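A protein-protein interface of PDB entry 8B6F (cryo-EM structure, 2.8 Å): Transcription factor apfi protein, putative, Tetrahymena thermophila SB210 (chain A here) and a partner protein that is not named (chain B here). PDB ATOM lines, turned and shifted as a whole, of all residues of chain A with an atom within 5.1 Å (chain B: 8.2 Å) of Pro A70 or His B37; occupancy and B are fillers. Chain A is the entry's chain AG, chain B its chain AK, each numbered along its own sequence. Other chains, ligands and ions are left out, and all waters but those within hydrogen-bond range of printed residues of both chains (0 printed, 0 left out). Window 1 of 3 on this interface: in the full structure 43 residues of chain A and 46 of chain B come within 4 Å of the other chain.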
ATOM      1  N   SER A  49       5.573  25.425   3.866  1.00  0.00           N
ATOM      2  CA  SER A  49       4.755  24.709   4.838  1.00  0.00           C
ATOM      3  C   SER A  49       5.201  23.253   4.862  1.00  0.00           C
ATOM      4  O   SER A  49       5.025  22.525   3.880  1.00  0.00           O
ATOM      5  CB  SER A  49       3.275  24.824   4.485  1.00  0.00           C
ATOM      6  OG  SER A  49       2.475  24.075   5.384  1.00  0.00           O
ATOM      7  N   LEU A  50       5.778  22.826   5.983  1.00  0.00           N
ATOM      8  CA  LEU A  50       6.332  21.486   6.100  1.00  0.00           C
ATOM      9  C   LEU A  50       5.337  20.481   6.658  1.00  0.00           C
ATOM     10  O   LEU A  50       5.714  19.332   6.908  1.00  0.00           O
ATOM     11  CB  LEU A  50       7.591  21.517   6.967  1.00  0.00           C
ATOM     12  CG  LEU A  50       8.697  22.444   6.448  1.00  0.00           C
ATOM     13  CD1 LEU A  50       9.909  22.363   7.343  1.00  0.00           C
ATOM     14  CD2 LEU A  50       9.082  22.114   5.009  1.00  0.00           C
ATOM     15  N   ARG A  51       4.091  20.884   6.879  1.00  0.00           N
ATOM     16  CA  ARG A  51       3.040  19.921   7.161  1.00  0.00           C
ATOM     17  C   ARG A  51       2.714  19.137   5.898  1.00  0.00           C
ATOM     18  O   ARG A  51       2.657  19.696   4.800  1.00  0.00           O
ATOM     19  CB  ARG A  51       1.783  20.627   7.665  1.00  0.00           C
ATOM     20  CG  ARG A  51       2.014  21.563   8.832  1.00  0.00           C
ATOM     21  CD  ARG A  51       0.713  22.200   9.278  1.00  0.00           C
ATOM     22  NE  ARG A  51       0.089  22.978   8.217  1.00  0.00           N
ATOM     23  CZ  ARG A  51      -1.009  23.707   8.369  1.00  0.00           C
ATOM     24  NH1 ARG A  51      -1.631  23.784   9.532  1.00  0.00           N
ATOM     25  NH2 ARG A  51      -1.491  24.376   7.327  1.00  0.00           N
ATOM     26  N   PHE A  67      -6.081  19.692  15.323  1.00  0.00           N
ATOM     27  CA  PHE A  67      -5.111  20.778  15.326  1.00  0.00           C
ATOM     28  C   PHE A  67      -3.758  20.267  14.861  1.00  0.00           C
ATOM     29  O   PHE A  67      -3.235  19.297  15.414  1.00  0.00           O
ATOM     30  CB  PHE A  67      -4.986  21.398  16.723  1.00  0.00           C
ATOM     31  CG  PHE A  67      -3.912  22.442  16.828  1.00  0.00           C
ATOM     32  CD1 PHE A  67      -3.951  23.576  16.039  1.00  0.00           C
ATOM     33  CD2 PHE A  67      -2.873  22.295  17.730  1.00  0.00           C
ATOM     34  CE1 PHE A  67      -2.968  24.540  16.139  1.00  0.00           C
ATOM     35  CE2 PHE A  67      -1.888  23.255  17.835  1.00  0.00           C
ATOM     36  CZ  PHE A  67      -1.936  24.378  17.038  1.00  0.00           C
ATOM     37  N   ILE A  68      -3.198  20.927  13.852  1.00  0.00           N
ATOM     38  CA  ILE A  68      -1.829  20.696  13.410  1.00  0.00           C
ATOM     39  C   ILE A  68      -1.152  22.055  13.353  1.00  0.00           C
ATOM     40  O   ILE A  68      -1.581  22.934  12.596  1.00  0.00           O
ATOM     41  CB  ILE A  68      -1.766  19.998  12.041  1.00  0.00           C
ATOM     42  CG1 ILE A  68      -2.610  18.718  12.040  1.00  0.00           C
ATOM     43  CG2 ILE A  68      -0.321  19.693  11.661  1.00  0.00           C
ATOM     44  CD1 ILE A  68      -2.080  17.612  12.928  1.00  0.00           C
ATOM     45  N   ALA A  69      -0.105  22.234  14.149  1.00  0.00           N
ATOM     46  CA  ALA A  69       0.536  23.536  14.232  1.00  0.00           C
ATOM     47  C   ALA A  69       1.123  23.917  12.876  1.00  0.00           C
ATOM     48  O   ALA A  69       1.710  23.069  12.194  1.00  0.00           O
ATOM     49  CB  ALA A  69       1.634  23.529  15.293  1.00  0.00           C
ATOM     50  N   PRO A  70       0.994  25.177  12.456  1.00  0.00           N
ATOM     51  CA  PRO A  70       1.486  25.549  11.122  1.00  0.00           C
ATOM     52  C   PRO A  70       2.977  25.331  10.938  1.00  0.00           C
ATOM     53  O   PRO A  70       3.415  25.049   9.816  1.00  0.00           O
ATOM     54  CB  PRO A  70       1.109  27.033  11.012  1.00  0.00           C
ATOM     55  CG  PRO A  70       0.995  27.502  12.411  1.00  0.00           C
ATOM     56  CD  PRO A  70       0.470  26.341  13.192  1.00  0.00           C
ATOM     57  N   ASN A  71       3.774  25.456  11.998  1.00  0.00           N
ATOM     58  CA  ASN A  71       5.223  25.333  11.905  1.00  0.00           C
ATOM     59  C   ASN A  71       5.727  23.952  12.310  1.00  0.00           C
ATOM     60  O   ASN A  71       6.936  23.770  12.474  1.00  0.00           O
ATOM     61  CB  ASN A  71       5.901  26.407  12.757  1.00  0.00           C
ATOM     62  CG  ASN A  71       5.600  26.260  14.230  1.00  0.00           C
ATOM     63  OD1 ASN A  71       4.550  25.750  14.614  1.00  0.00           O
ATOM     64  ND2 ASN A  71       6.523  26.711  15.068  1.00  0.00           N
ATOM     65  N   SER A  72       4.835  22.982  12.482  1.00  0.00           N
ATOM     66  CA  SER A  72       5.255  21.620  12.760  1.00  0.00           C
ATOM     67  C   SER A  72       5.755  20.954  11.480  1.00  0.00           C
ATOM     68  O   SER A  72       5.602  21.475  10.374  1.00  0.00           O
ATOM     69  CB  SER A  72       4.109  20.816  13.372  1.00  0.00           C
ATOM     70  OG  SER A  72       3.027  20.699  12.468  1.00  0.00           O
ATOM     71  N   TYR A  88       3.049  23.034  18.262  1.00  0.00           N
ATOM     72  CA  TYR A  88       4.083  23.812  17.591  1.00  0.00           C
ATOM     73  C   TYR A  88       5.440  23.127  17.653  1.00  0.00           C
ATOM     74  O   TYR A  88       5.872  22.665  18.712  1.00  0.00           O
ATOM     75  CB  TYR A  88       4.174  25.200  18.223  1.00  0.00           C
ATOM     76  CG  TYR A  88       2.868  25.953  18.193  1.00  0.00           C
ATOM     77  CD1 TYR A  88       2.531  26.745  17.105  1.00  0.00           C
ATOM     78  CD2 TYR A  88       1.972  25.868  19.247  1.00  0.00           C
ATOM     79  CE1 TYR A  88       1.340  27.432  17.067  1.00  0.00           C
ATOM     80  CE2 TYR A  88       0.777  26.551  19.219  1.00  0.00           C
ATOM     81  CZ  TYR A  88       0.468  27.333  18.125  1.00  0.00           C
ATOM     82  OH  TYR A  88      -0.719  28.019  18.086  1.00  0.00           O
ATOM     83  N   THR A 220      -5.065  29.603  14.536  1.00  0.00           N
ATOM     84  CA  THR A 220      -4.018  29.463  13.529  1.00  0.00           C
ATOM     85  C   THR A 220      -4.597  29.432  12.121  1.00  0.00           C
ATOM     86  O   THR A 220      -4.037  30.038  11.201  1.00  0.00           O
ATOM     87  CB  THR A 220      -3.197  28.201  13.792  1.00  0.00           C
ATOM     88  OG1 THR A 220      -4.070  27.073  13.913  1.00  0.00           O
ATOM     89  CG2 THR A 220      -2.378  28.350  15.062  1.00  0.00           C
ATOM     90  N   TYR B  30      -4.699  20.846   5.336  1.00  0.00           N
ATOM     91  CA  TYR B  30      -3.340  21.282   5.626  1.00  0.00           C
ATOM     92  C   TYR B  30      -2.463  21.260   4.378  1.00  0.00           C
ATOM     93  O   TYR B  30      -1.245  21.102   4.473  1.00  0.00           O
ATOM     94  CB  TYR B  30      -2.730  20.410   6.723  1.00  0.00           C
ATOM     95  CG  TYR B  30      -3.687  20.121   7.855  1.00  0.00           C
ATOM     96  CD1 TYR B  30      -4.032  21.105   8.772  1.00  0.00           C
ATOM     97  CD2 TYR B  30      -4.239  18.858   8.011  1.00  0.00           C
ATOM     98  CE1 TYR B  30      -4.905  20.841   9.807  1.00  0.00           C
ATOM     99  CE2 TYR B  30      -5.113  18.583   9.043  1.00  0.00           C
ATOM    100  CZ  TYR B  30      -5.440  19.579   9.938  1.00  0.00           C
ATOM    101  OH  TYR B  30      -6.311  19.305  10.965  1.00  0.00           O
ATOM    102  N   GLU B  32      -0.889  23.364   1.610  1.00  0.00           N
ATOM    103  CA  GLU B  32      -0.515  24.650   1.037  1.00  0.00           C
ATOM    104  C   GLU B  32       1.003  24.719   0.984  1.00  0.00           C
ATOM    105  O   GLU B  32       1.700  23.944   1.643  1.00  0.00           O
ATOM    106  CB  GLU B  32      -1.096  25.827   1.834  1.00  0.00           C
ATOM    107  CG  GLU B  32      -0.418  26.114   3.170  1.00  0.00           C
ATOM    108  CD  GLU B  32      -0.573  24.987   4.166  1.00  0.00           C
ATOM    109  OE1 GLU B  32      -1.378  24.068   3.905  1.00  0.00           O
ATOM    110  OE2 GLU B  32       0.108  25.017   5.211  1.00  0.00           O
ATOM    111  N   ILE B  34       2.849  27.798   1.354  1.00  0.00           N
ATOM    112  CA  ILE B  34       3.383  28.866   2.193  1.00  0.00           C
ATOM    113  C   ILE B  34       2.871  28.659   3.610  1.00  0.00           C
ATOM    114  O   ILE B  34       1.666  28.493   3.826  1.00  0.00           O
ATOM    115  CB  ILE B  34       2.985  30.253   1.660  1.00  0.00           C
ATOM    116  CG1 ILE B  34       3.441  30.405   0.205  1.00  0.00           C
ATOM    117  CG2 ILE B  34       3.590  31.347   2.531  1.00  0.00           C
ATOM    118  CD1 ILE B  34       3.008  31.699  -0.450  1.00  0.00           C
ATOM    119  N   SER B  35       3.791  28.668   4.571  1.00  0.00           N
ATOM    120  CA  SER B  35       3.424  28.454   5.963  1.00  0.00           C
ATOM    121  C   SER B  35       2.515  29.571   6.459  1.00  0.00           C
ATOM    122  O   SER B  35       2.660  30.734   6.073  1.00  0.00           O
ATOM    123  CB  SER B  35       4.680  28.377   6.831  1.00  0.00           C
ATOM    124  OG  SER B  35       4.349  28.243   8.201  1.00  0.00           O
ATOM    125  N   LYS B  36       1.574  29.208   7.329  1.00  0.00           N
ATOM    126  CA  LYS B  36       0.640  30.150   7.942  1.00  0.00           C
ATOM    127  C   LYS B  36       1.016  30.448   9.386  1.00  0.00           C
ATOM    128  O   LYS B  36       0.144  30.608  10.244  1.00  0.00           O
ATOM    129  CB  LYS B  36      -0.782  29.602   7.865  1.00  0.00           C
ATOM    130  CG  LYS B  36      -1.270  29.343   6.451  1.00  0.00           C
ATOM    131  CD  LYS B  36      -2.608  28.616   6.441  1.00  0.00           C
ATOM    132  CE  LYS B  36      -3.719  29.445   7.069  1.00  0.00           C
ATOM    133  NZ  LYS B  36      -3.912  30.753   6.383  1.00  0.00           N
ATOM    134  N   HIS B  37       2.310  30.528   9.680  1.00  0.00           N
ATOM    135  CA  HIS B  37       2.802  30.665  11.042  1.00  0.00           C
ATOM    136  C   HIS B  37       3.076  32.125  11.372  1.00  0.00           C
ATOM    137  O   HIS B  37       3.669  32.854  10.571  1.00  0.00           O
ATOM    138  CB  HIS B  37       4.077  29.843  11.237  1.00  0.00           C
ATOM    139  CG  HIS B  37       4.706  30.018  12.583  1.00  0.00           C
ATOM    140  ND1 HIS B  37       5.784  30.851  12.796  1.00  0.00           N
ATOM    141  CD2 HIS B  37       4.408  29.473  13.785  1.00  0.00           C
ATOM    142  CE1 HIS B  37       6.123  30.810  14.072  1.00  0.00           C
ATOM    143  NE2 HIS B  37       5.304  29.981  14.694  1.00  0.00           N
ATOM    144  N   ARG B  38       2.638  32.544  12.558  1.00  0.00           N
ATOM    145  CA  ARG B  38       2.882  33.883  13.074  1.00  0.00           C
ATOM    146  C   ARG B  38       3.536  33.782  14.443  1.00  0.00           C
ATOM    147  O   ARG B  38       3.132  32.962  15.272  1.00  0.00           O
ATOM    148  CB  ARG B  38       1.584  34.684  13.179  1.00  0.00           C
ATOM    149  CG  ARG B  38       0.922  34.966  11.842  1.00  0.00           C
ATOM    150  CD  ARG B  38      -0.474  35.516  12.040  1.00  0.00           C
ATOM    151  NE  ARG B  38      -1.351  34.530  12.656  1.00  0.00           N
ATOM    152  CZ  ARG B  38      -2.540  34.802  13.173  1.00  0.00           C
ATOM    153  NH1 ARG B  38      -3.024  36.031  13.184  1.00  0.00           N
ATOM    154  NH2 ARG B  38      -3.261  33.814  13.695  1.00  0.00           N
ATOM    155  N   SER B  39       4.553  34.613  14.673  1.00  0.00           N
ATOM    156  CA  SER B  39       5.249  34.587  15.956  1.00  0.00           C
ATOM    157  C   SER B  39       4.335  35.015  17.096  1.00  0.00           C
ATOM    158  O   SER B  39       4.316  34.379  18.155  1.00  0.00           O
ATOM    159  CB  SER B  39       6.480  35.489  15.902  1.00  0.00           C
ATOM    160  OG  SER B  39       7.375  35.074  14.888  1.00  0.00           O
ATOM    161  N   LEU B  40       3.572  36.085  16.901  1.00  0.00           N
ATOM    162  CA  LEU B  40       2.693  36.629  17.926  1.00  0.00           C
ATOM    163  C   LEU B  40       1.250  36.304  17.574  1.00  0.00           C
ATOM    164  O   LEU B  40       0.816  36.532  16.441  1.00  0.00           O
ATOM    165  CB  LEU B  40       2.875  38.143  18.061  1.00  0.00           C
ATOM    166  CG  LEU B  40       4.295  38.635  18.354  1.00  0.00           C
ATOM    167  CD1 LEU B  40       4.298  40.138  18.564  1.00  0.00           C
ATOM    168  CD2 LEU B  40       4.893  37.930  19.557  1.00  0.00           C
ATOM    169  N   MET B  41       0.514  35.777  18.548  1.00  0.00           N
ATOM    170  CA  MET B  41      -0.877  35.406  18.343  1.00  0.00           C
ATOM    171  C   MET B  41      -1.635  35.619  19.643  1.00  0.00           C
ATOM    172  O   MET B  41      -1.045  35.716  20.721  1.00  0.00           O
ATOM    173  CB  MET B  41      -1.007  33.954  17.874  1.00  0.00           C
ATOM    174  CG  MET B  41      -0.517  33.723  16.450  1.00  0.00           C
ATOM    175  SD  MET B  41      -0.612  31.997  15.937  1.00  0.00           S
ATOM    176  CE  MET B  41       0.722  31.277  16.893  1.00  0.00           C
ATOM    177  N   ALA B  57      12.431  35.879  17.996  1.00  0.00           N
ATOM    178  CA  ALA B  57      12.845  35.287  16.738  1.00  0.00           C
ATOM    179  C   ALA B  57      11.626  34.927  15.889  1.00  0.00           C
ATOM    180  O   ALA B  57      10.585  34.534  16.421  1.00  0.00           O
ATOM    181  CB  ALA B  57      13.684  34.040  16.987  1.00  0.00           C
ATOM    182  N   PRO B  58      11.726  35.051  14.562  1.00  0.00           N
ATOM    183  CA  PRO B  58      10.583  34.664  13.718  1.00  0.00           C
ATOM    184  C   PRO B  58      10.167  33.216  13.906  1.00  0.00           C
ATOM    185  O   PRO B  58       8.974  32.902  13.835  1.00  0.00           O
ATOM    186  CB  PRO B  58      11.093  34.935  12.296  1.00  0.00           C
ATOM    187  CG  PRO B  58      12.169  35.940  12.460  1.00  0.00           C
ATOM    188  CD  PRO B  58      12.825  35.623  13.764  1.00  0.00           C
ATOM    189  N   ASN B  59      11.127  32.319  14.137  1.00  0.00           N
ATOM    190  CA  ASN B  59      10.789  30.930  14.429  1.00  0.00           C
ATOM    191  C   ASN B  59       9.993  30.814  15.721  1.00  0.00           C
ATOM    192  O   ASN B  59       9.069  29.999  15.819  1.00  0.00           O
ATOM    193  CB  ASN B  59      12.064  30.090  14.523  1.00  0.00           C
ATOM    194  CG  ASN B  59      12.394  29.383  13.231  1.00  0.00           C
ATOM    195  OD1 ASN B  59      11.775  29.631  12.197  1.00  0.00           O
ATOM    196  ND2 ASN B  59      13.374  28.488  13.281  1.00  0.00           N
ATOM    197  N   SER B  60      10.344  31.612  16.724  1.00  0.00           N
ATOM    198  CA  SER B  60       9.711  31.506  18.031  1.00  0.00           C
ATOM    199  C   SER B  60       8.231  31.856  17.956  1.00  0.00           C
ATOM    200  O   SER B  60       7.811  32.723  17.187  1.00  0.00           O
ATOM    201  CB  SER B  60      10.405  32.431  19.031  1.00  0.00           C
ATOM    202  OG  SER B  60      11.770  32.087  19.184  1.00  0.00           O
ATOM    203  N   THR B  61       7.437  31.168  18.772  1.00  0.00           N
ATOM    204  CA  THR B  61       6.009  31.420  18.891  1.00  0.00           C
ATOM    205  C   THR B  61       5.711  31.971  20.279  1.00  0.00           C
ATOM    206  O   THR B  61       6.149  31.401  21.283  1.00  0.00           O
ATOM    207  CB  THR B  61       5.205  30.141  18.654  1.00  0.00           C
ATOM    208  OG1 THR B  61       5.559  29.576  17.386  1.00  0.00           O
ATOM    209  CG2 THR B  61       3.711  30.435  18.675  1.00  0.00           C
ATOM    210  N   VAL B  62       4.963  33.069  20.333  1.00  0.00           N
ATOM    211  CA  VAL B  62       4.558  33.698  21.587  1.00  0.00           C
ATOM    212  C   VAL B  62       3.061  33.954  21.471  1.00  0.00           C
ATOM    213  O   VAL B  62       2.643  34.966  20.898  1.00  0.00           O
ATOM    214  CB  VAL B  62       5.321  34.997  21.865  1.00  0.00           C
ATOM    215  CG1 VAL B  62       4.843  35.633  23.160  1.00  0.00           C
ATOM    216  CG2 VAL B  62       6.816  34.735  21.913  1.00  0.00           C
ATOM    217  N   ASN B  77      12.984  29.049  17.650  1.00  0.00           N
ATOM    218  CA  ASN B  77      12.333  27.760  17.880  1.00  0.00           C
ATOM    219  C   ASN B  77      11.928  27.573  19.342  1.00  0.00           C
ATOM    220  O   ASN B  77      12.009  26.470  19.878  1.00  0.00           O
ATOM    221  CB  ASN B  77      13.232  26.609  17.423  1.00  0.00           C
ATOM    222  CG  ASN B  77      12.457  25.335  17.161  1.00  0.00           C
ATOM    223  OD1 ASN B  77      11.416  25.092  17.768  1.00  0.00           O
ATOM    224  ND2 ASN B  77      12.961  24.513  16.250  1.00  0.00           N
ATOM    225  N   SER B  78      11.486  28.648  19.988  1.00  0.00           N
ATOM    226  CA  SER B  78      11.016  28.600  21.364  1.00  0.00           C
ATOM    227  C   SER B  78       9.533  28.940  21.407  1.00  0.00           C
ATOM    228  O   SER B  78       9.079  29.854  20.714  1.00  0.00           O
ATOM    229  CB  SER B  78      11.798  29.570  22.251  1.00  0.00           C
ATOM    230  OG  SER B  78      13.183  29.275  22.230  1.00  0.00           O
ATOM    231  N   VAL B  79       8.783  28.200  22.220  1.00  0.00           N
ATOM    232  CA  VAL B  79       7.333  28.335  22.309  1.00  0.00           C
ATOM    233  C   VAL B  79       6.971  28.871  23.687  1.00  0.00           C
ATOM    234  O   VAL B  79       7.440  28.350  24.706  1.00  0.00           O
ATOM    235  CB  VAL B  79       6.626  26.996  22.041  1.00  0.00           C
ATOM    236  CG1 VAL B  79       5.118  27.175  22.091  1.00  0.00           C
ATOM    237  CG2 VAL B  79       7.054  26.426  20.700  1.00  0.00           C
ATOM    238  N   TYR B 257       4.189  43.855  12.930  1.00  0.00           N
ATOM    239  CA  TYR B 257       3.179  43.781  11.880  1.00  0.00           C
ATOM    240  C   TYR B 257       2.815  45.175  11.382  1.00  0.00           C
ATOM    241  O   TYR B 257       2.241  45.974  12.119  1.00  0.00           O
ATOM    242  CB  TYR B 257       1.925  43.066  12.388  1.00  0.00           C
ATOM    243  CG  TYR B 257       2.164  41.648  12.860  1.00  0.00           C
ATOM    244  CD1 TYR B 257       3.183  40.873  12.320  1.00  0.00           C
ATOM    245  CD2 TYR B 257       1.369  41.085  13.847  1.00  0.00           C
ATOM    246  CE1 TYR B 257       3.402  39.578  12.750  1.00  0.00           C
ATOM    247  CE2 TYR B 257       1.580  39.792  14.285  1.00  0.00           C
ATOM    248  CZ  TYR B 257       2.597  39.045  13.732  1.00  0.00           C
ATOM    249  OH  TYR B 257       2.808  37.759  14.165  1.00  0.00           O
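Among the printed residues, merely in contact across the chains: Ser A49 with Ile B34 (3.95 Å), Ser A49 with Ser B35 (3.8 Å), Arg A51 with Tyr B30 (3.7 Å), Ile A68 with Tyr B30 (3.6 Å), Pro A70 with Ser B35 (3.7 Å), Pro A70 with Lys B36 (3.8 Å), Pro A70 with His B37 (3.9 Å), Asn A71 with His B37 (3.5 Å), Asn A71 with Thr B61 (3.8 Å), Tyr A88 with Met B41 (3.8 Å) and Tyr A88 with Val B79 (3.99 Å).
The guanidinium group (NH1) of Arg A51 sits at hydrogen-bond distance from the backbone carbonyl oxygen (O) of Ile A68 (3.2 Å). OG of Ser B35 sits close to N of His B37 (3.4 Å). A ring nitrogen (NE2) of His B37 is in hydrogen-bond range of the side-chain hydroxyl of Thr B61 (2.7 Å). The backbone NH of Met B41 is in hydrogen-bond range of the backbone carbonyl oxygen of Val B62. The backbone carbonyl oxygen of Ser B78 sits at hydrogen-bond distance from the backbone NH of Thr B61 (2.9 Å).
Printed residues of chain B within 4 Å of Pro A70: Ser B35 (3.7 Å), Lys B36 (3.8 Å) and His B37 (3.9 Å). Of the printed residues of chain A, His B37 touches Pro A70 (3.9 Å) and Asn A71 (3.5 Å). Of the printed residues of chain B, Asn A71 touches His B37 (3.5 Å) and Thr B61 (3.8 Å). Printed residues of chain A within 4 Å of Met B41: Tyr A88. Of the printed residues of chain A, Val B79 touches Tyr A88 (3.99 Å). Of the printed residues of chain B, Tyr A88 touches Met B41 (3.8 Å) and Val B79 (3.99 Å).
Of the 11 printed residues of chain A, 6 touch a printed residue of chain B. Printed residues of chain A that touch a printed residue of chain B: Ser A49, Arg A51, Ile A68, Pro A70, Asn A71 and Tyr A88. Hydrophobic or aromatic side chains of chain A that line the printed part of chain B: Ile A68, Pro A70 and Tyr A88. Along chain B the printed residues that touch a printed residue of chain A span positions 30 to 79. Among the printed residues, 13 pairs touch across the chains. Among the printed residues, Asp or Glu carboxylates within 4 Å of a Lys or Arg side-chain nitrogen of the other chain: Arg A51 with Glu B32.
The side-chain hydroxyl of Ser A49 lies within hydrogen-bond range of the side-chain carboxylate of Glu B32. NH2 of Arg A51 is in salt-bridge range of OE2 of Glu B32 (2.7 Å).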
